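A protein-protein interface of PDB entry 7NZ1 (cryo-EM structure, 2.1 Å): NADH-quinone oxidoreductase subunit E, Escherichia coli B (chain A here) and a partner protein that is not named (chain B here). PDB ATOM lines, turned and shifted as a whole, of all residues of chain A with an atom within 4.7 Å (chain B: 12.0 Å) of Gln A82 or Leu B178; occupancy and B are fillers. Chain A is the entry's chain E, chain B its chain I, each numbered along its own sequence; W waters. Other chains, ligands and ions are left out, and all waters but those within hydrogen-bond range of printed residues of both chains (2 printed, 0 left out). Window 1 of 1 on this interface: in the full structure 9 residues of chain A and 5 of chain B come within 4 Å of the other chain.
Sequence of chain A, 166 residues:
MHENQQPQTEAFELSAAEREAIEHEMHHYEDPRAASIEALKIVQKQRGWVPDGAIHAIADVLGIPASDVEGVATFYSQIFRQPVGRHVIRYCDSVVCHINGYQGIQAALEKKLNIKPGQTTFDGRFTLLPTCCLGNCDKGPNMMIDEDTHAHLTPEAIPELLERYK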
ATOM      1  N   TRP A  49      37.086  13.321  17.502  1.00  0.00           N
ATOM      2  CA  TRP A  49      35.633  13.251  17.501  1.00  0.00           C
ATOM      3  C   TRP A  49      35.155  13.662  18.886  1.00  0.00           C
ATOM      4  O   TRP A  49      35.951  13.807  19.814  1.00  0.00           O
ATOM      5  CB  TRP A  49      35.148  11.849  17.106  1.00  0.00           C
ATOM      6  CG  TRP A  49      35.446  10.778  18.115  1.00  0.00           C
ATOM      7  CD1 TRP A  49      36.677  10.328  18.505  1.00  0.00           C
ATOM      8  CD2 TRP A  49      34.491  10.001  18.840  1.00  0.00           C
ATOM      9  NE1 TRP A  49      36.546   9.335  19.437  1.00  0.00           N
ATOM     10  CE2 TRP A  49      35.214   9.111  19.660  1.00  0.00           C
ATOM     11  CE3 TRP A  49      33.095   9.969  18.877  1.00  0.00           C
ATOM     12  CZ2 TRP A  49      34.586   8.205  20.511  1.00  0.00           C
ATOM     13  CZ3 TRP A  49      32.476   9.076  19.717  1.00  0.00           C
ATOM     14  CH2 TRP A  49      33.221   8.203  20.525  1.00  0.00           C
ATOM     15  N   PHE A  80      31.450  15.348  14.779  1.00  0.00           N
ATOM     16  CA  PHE A  80      31.405  13.893  14.671  1.00  0.00           C
ATOM     17  C   PHE A  80      31.080  13.266  16.021  1.00  0.00           C
ATOM     18  O   PHE A  80      31.709  13.590  17.032  1.00  0.00           O
ATOM     19  CB  PHE A  80      32.736  13.334  14.158  1.00  0.00           C
ATOM     20  CG  PHE A  80      33.154  13.864  12.810  1.00  0.00           C
ATOM     21  CD1 PHE A  80      32.270  13.868  11.743  1.00  0.00           C
ATOM     22  CD2 PHE A  80      34.446  14.326  12.607  1.00  0.00           C
ATOM     23  CE1 PHE A  80      32.656  14.346  10.500  1.00  0.00           C
ATOM     24  CE2 PHE A  80      34.840  14.807  11.369  1.00  0.00           C
ATOM     25  CZ  PHE A  80      33.943  14.811  10.312  1.00  0.00           C
ATOM     26  N   ARG A  81      30.135  12.327  16.017  1.00  0.00           N
ATOM     27  CA  ARG A  81      29.734  11.600  17.216  1.00  0.00           C
ATOM     28  C   ARG A  81      30.063  10.115  17.117  1.00  0.00           C
ATOM     29  O   ARG A  81      29.550   9.320  17.908  1.00  0.00           O
ATOM     30  CB  ARG A  81      28.240  11.807  17.490  1.00  0.00           C
ATOM     31  CG  ARG A  81      27.876  13.215  17.964  1.00  0.00           C
ATOM     32  CD  ARG A  81      28.218  13.496  19.429  1.00  0.00           C
ATOM     33  NE  ARG A  81      27.437  12.686  20.359  1.00  0.00           N
ATOM     34  CZ  ARG A  81      27.874  11.590  20.965  1.00  0.00           C
ATOM     35  NH1 ARG A  81      29.105  11.143  20.784  1.00  0.00           N
ATOM     36  NH2 ARG A  81      27.048  10.914  21.760  1.00  0.00           N
ATOM     37  N   GLN A  82      30.896   9.729  16.159  1.00  0.00           N
ATOM     38  CA  GLN A  82      31.409   8.386  15.959  1.00  0.00           C
ATOM     39  C   GLN A  82      32.905   8.490  15.695  1.00  0.00           C
ATOM     40  O   GLN A  82      33.361   9.505  15.163  1.00  0.00           O
ATOM     41  CB  GLN A  82      30.688   7.693  14.790  1.00  0.00           C
ATOM     42  CG  GLN A  82      29.459   6.911  15.234  1.00  0.00           C
ATOM     43  CD  GLN A  82      28.502   6.590  14.106  1.00  0.00           C
ATOM     44  OE1 GLN A  82      28.861   6.654  12.934  1.00  0.00           O
ATOM     45  NE2 GLN A  82      27.269   6.246  14.460  1.00  0.00           N
ATOM     46  N   PRO A  83      33.697   7.489  16.107  1.00  0.00           N
ATOM     47  CA  PRO A  83      35.156   7.587  15.937  1.00  0.00           C
ATOM     48  C   PRO A  83      35.575   7.544  14.475  1.00  0.00           C
ATOM     49  O   PRO A  83      35.049   6.767  13.679  1.00  0.00           O
ATOM     50  CB  PRO A  83      35.692   6.374  16.708  1.00  0.00           C
ATOM     51  CG  PRO A  83      34.579   5.942  17.582  1.00  0.00           C
ATOM     52  CD  PRO A  83      33.327   6.280  16.862  1.00  0.00           C
ATOM     53  N   VAL A  84      36.517   8.415  14.132  1.00  0.00           N
ATOM     54  CA  VAL A  84      36.982   8.569  12.763  1.00  0.00           C
ATOM     55  C   VAL A  84      38.445   8.161  12.687  1.00  0.00           C
ATOM     56  O   VAL A  84      39.048   7.772  13.691  1.00  0.00           O
ATOM     57  CB  VAL A  84      36.789  10.016  12.279  1.00  0.00           C
ATOM     58  CG1 VAL A  84      35.315  10.317  12.120  1.00  0.00           C
ATOM     59  CG2 VAL A  84      37.429  10.989  13.250  1.00  0.00           C
ATOM     60  N   GLY A 118      31.649   6.530   4.447  1.00  0.00           N
ATOM     61  CA  GLY A 118      31.112   6.379   5.777  1.00  0.00           C
ATOM     62  C   GLY A 118      31.883   5.403   6.641  1.00  0.00           C
ATOM     63  O   GLY A 118      31.628   5.331   7.849  1.00  0.00           O
ATOM     64  N   THR A 127      39.290   7.759   7.050  1.00  0.00           N
ATOM     65  CA  THR A 127      37.841   7.619   6.953  1.00  0.00           C
ATOM     66  C   THR A 127      37.371   8.385   5.717  1.00  0.00           C
ATOM     67  O   THR A 127      37.855   9.487   5.438  1.00  0.00           O
ATOM     68  CB  THR A 127      37.125   8.084   8.239  1.00  0.00           C
ATOM     69  OG1 THR A 127      35.705   7.978   8.078  1.00  0.00           O
ATOM     70  CG2 THR A 127      37.502   9.491   8.637  1.00  0.00           C
ATOM     71  N   LEU A 129      34.407  10.098   3.463  1.00  0.00           N
ATOM     72  CA  LEU A 129      33.104  10.738   3.609  1.00  0.00           C
ATOM     73  C   LEU A 129      32.776  11.623   2.409  1.00  0.00           C
ATOM     74  O   LEU A 129      33.631  12.406   1.974  1.00  0.00           O
ATOM     75  CB  LEU A 129      33.068  11.573   4.893  1.00  0.00           C
ATOM     76  CG  LEU A 129      32.568  10.860   6.148  1.00  0.00           C
ATOM     77  CD1 LEU A 129      32.793  11.720   7.381  1.00  0.00           C
ATOM     78  CD2 LEU A 129      31.108  10.491   6.003  1.00  0.00           C
ATOM     79  N   PRO B 172      17.679   0.856  10.157  1.00  0.00           N
ATOM     80  CA  PRO B 172      17.695   2.073  10.987  1.00  0.00           C
ATOM     81  C   PRO B 172      19.040   2.785  10.904  1.00  0.00           C
ATOM     82  O   PRO B 172      20.098   2.167  11.041  1.00  0.00           O
ATOM     83  CB  PRO B 172      17.427   1.551  12.404  1.00  0.00           C
ATOM     84  CG  PRO B 172      16.985   0.152  12.251  1.00  0.00           C
ATOM     85  CD  PRO B 172      17.538  -0.363  10.972  1.00  0.00           C
ATOM     86  N   ILE B 173      18.989   4.094  10.680  1.00  0.00           N
ATOM     87  CA  ILE B 173      20.171   4.948  10.660  1.00  0.00           C
ATOM     88  C   ILE B 173      20.197   5.755  11.946  1.00  0.00           C
ATOM     89  O   ILE B 173      19.234   6.462  12.264  1.00  0.00           O
ATOM     90  CB  ILE B 173      20.180   5.880   9.436  1.00  0.00           C
ATOM     91  CG1 ILE B 173      19.779   5.108   8.177  1.00  0.00           C
ATOM     92  CG2 ILE B 173      21.531   6.586   9.310  1.00  0.00           C
ATOM     93  CD1 ILE B 173      20.000   5.850   6.885  1.00  0.00           C
ATOM     94  N   ASP B 174      21.304   5.664  12.674  1.00  0.00           N
ATOM     95  CA  ASP B 174      21.439   6.415  13.908  1.00  0.00           C
ATOM     96  C   ASP B 174      21.687   7.884  13.590  1.00  0.00           C
ATOM     97  O   ASP B 174      22.255   8.228  12.551  1.00  0.00           O
ATOM     98  CB  ASP B 174      22.585   5.850  14.745  1.00  0.00           C
ATOM     99  CG  ASP B 174      22.482   6.221  16.217  1.00  0.00           C
ATOM    100  OD1 ASP B 174      22.584   7.414  16.558  1.00  0.00           O
ATOM    101  OD2 ASP B 174      22.308   5.297  17.037  1.00  0.00           O
ATOM    102  N   VAL B 175      21.269   8.755  14.512  1.00  0.00           N
ATOM    103  CA  VAL B 175      21.533  10.183  14.383  1.00  0.00           C
ATOM    104  C   VAL B 175      23.018  10.507  14.505  1.00  0.00           C
ATOM    105  O   VAL B 175      23.454  11.562  14.035  1.00  0.00           O
ATOM    106  CB  VAL B 175      20.706  10.976  15.411  1.00  0.00           C
ATOM    107  CG1 VAL B 175      19.265  11.054  14.956  1.00  0.00           C
ATOM    108  CG2 VAL B 175      20.794  10.332  16.778  1.00  0.00           C
ATOM    109  N   LYS B 176      23.802   9.635  15.134  1.00  0.00           N
ATOM    110  CA  LYS B 176      25.229   9.854  15.318  1.00  0.00           C
ATOM    111  C   LYS B 176      26.060   9.418  14.115  1.00  0.00           C
ATOM    112  O   LYS B 176      27.289   9.551  14.165  1.00  0.00           O
ATOM    113  CB  LYS B 176      25.717   9.115  16.568  1.00  0.00           C
ATOM    114  CG  LYS B 176      24.950   9.449  17.836  1.00  0.00           C
ATOM    115  CD  LYS B 176      25.707   9.023  19.084  1.00  0.00           C
ATOM    116  CE  LYS B 176      26.024   7.535  19.099  1.00  0.00           C
ATOM    117  NZ  LYS B 176      24.830   6.676  18.881  1.00  0.00           N
ATOM    118  N   SER B 177      25.423   8.872  13.071  1.00  0.00           N
ATOM    119  CA  SER B 177      26.118   8.397  11.874  1.00  0.00           C
ATOM    120  C   SER B 177      26.886   9.509  11.162  1.00  0.00           C
ATOM    121  O   SER B 177      26.450  10.662  11.114  1.00  0.00           O
ATOM    122  CB  SER B 177      25.128   7.754  10.904  1.00  0.00           C
ATOM    123  OG  SER B 177      24.175   8.692  10.441  1.00  0.00           O
ATOM    124  N   LEU B 178      28.059   9.148  10.632  1.00  0.00           N
ATOM    125  CA  LEU B 178      28.943  10.126  10.005  1.00  0.00           C
ATOM    126  C   LEU B 178      28.398  10.624   8.674  1.00  0.00           C
ATOM    127  O   LEU B 178      28.708  11.747   8.265  1.00  0.00           O
ATOM    128  CB  LEU B 178      30.331   9.525   9.797  1.00  0.00           C
ATOM    129  CG  LEU B 178      31.061   9.089  11.065  1.00  0.00           C
ATOM    130  CD1 LEU B 178      32.185   8.119  10.746  1.00  0.00           C
ATOM    131  CD2 LEU B 178      31.572  10.292  11.826  1.00  0.00           C
ATOM    132  N   LEU B 179      27.615   9.804   7.984  1.00  0.00           N
ATOM    133  CA  LEU B 179      27.111  10.178   6.669  1.00  0.00           C
ATOM    134  C   LEU B 179      26.015  11.226   6.813  1.00  0.00           C
ATOM    135  O   LEU B 179      25.135  11.078   7.669  1.00  0.00           O
ATOM    136  CB  LEU B 179      26.564   8.961   5.926  1.00  0.00           C
ATOM    137  CG  LEU B 179      27.559   7.903   5.446  1.00  0.00           C
ATOM    138  CD1 LEU B 179      26.856   6.572   5.274  1.00  0.00           C
ATOM    139  CD2 LEU B 179      28.241   8.327   4.157  1.00  0.00           C
ATOM    140  N   PRO B 180      26.041  12.304   6.016  1.00  0.00           N
ATOM    141  CA  PRO B 180      24.991  13.326   6.042  1.00  0.00           C
ATOM    142  C   PRO B 180      23.771  12.949   5.202  1.00  0.00           C
ATOM    143  O   PRO B 180      23.262  11.838   5.335  1.00  0.00           O
ATOM    144  CB  PRO B 180      25.697  14.548   5.463  1.00  0.00           C
ATOM    145  CG  PRO B 180      26.663  13.972   4.492  1.00  0.00           C
ATOM    146  CD  PRO B 180      27.122  12.655   5.077  1.00  0.00           C
HETATM  147  O   HOH W   1      28.682  12.152  13.632  1.00  0.00           O
HETATM  148  O   HOH W   2      28.671   6.688   8.638  1.00  0.00           O
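Along chain A the printed residues that touch a printed residue of chain B span positions 80 to 129.
Hydrophobic or aromatic side chains of chain B that line the printed part of chain A: Leu B178 and Leu B179.
Among the printed residues, 8 pairs touch across the chains.
Among the printed residues, no Asp or Glu carboxylate lies within 4 Å of a Lys or Arg side-chain nitrogen of the other chain.
Water W1 lies within hydrogen-bond range of the backbone NH of Arg A81 (2.8 Å) and the backbone carbonyl oxygen of Lys B176 (3.0 Å).
Water W2 lies within hydrogen-bond range of the backbone NH of Leu B178 (3.2 Å), the backbone carbonyl oxygen of Gly A118 (3.3 Å) and the backbone NH of Leu B179 (3.4 Å).
Gln A82 touches just these residues of chain B: Lys B176 (3.2 Å), Ser B177 (3.4 Å) and Leu B178 (3.5 Å).
Trp A49 touches none of the printed residues of chain B.
Phe A80 touches just one residue of chain B: Leu B178.
Of the printed residues of chain B, Arg A81 touches Lys B176.
No residue of chain B comes within 4 Å of Pro A83.
Of chain B, only Leu B179 (3.8 Å) comes within 4 Å of Gly A118.
Of the printed residues of chain A, Leu B179 touches Gly A118 (3.8 Å).
Printed residues of chain A within 4 Å of Ser B177: Gln A82 (3.4 Å).
Of the printed residues of chain B, Leu A129 touches Leu B178.
Printed residues of chain A within 4 Å of Lys B176: Arg A81 (3.5 Å) and Gln A82 (3.2 Å).
Asp B174 touches none of the printed residues of chain A.
The nearest residue of chain B that does not touch Gln A82 is Asp B174 (4.7 Å).
The side-chain amino group of Lys B176 is in salt-bridge range of the side-chain carboxylate of Asp B174, at 3.3 Å.
O of Asp B174 sits at hydrogen-bond distance from OG of Ser B177.
The side-chain amide oxygen (OE1) of Gln A82 sits at hydrogen-bond distance from the backbone NH (N) of Leu B178 (3.5 Å).
The backbone NH (N) of Ser B177 sits close to the side-chain amide nitrogen (NE2) of Gln A82.
The side-chain amide nitrogen (NE2) of Gln A82 sits close to the backbone carbonyl oxygen (O) of Lys B176.
Among the printed residues, merely in contact across the chains: Leu A129 with Leu B178, Arg A81 with Lys B176, Phe A80 with Leu B178, Val A84 with Leu B178 and Gly A118 with Leu B179.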
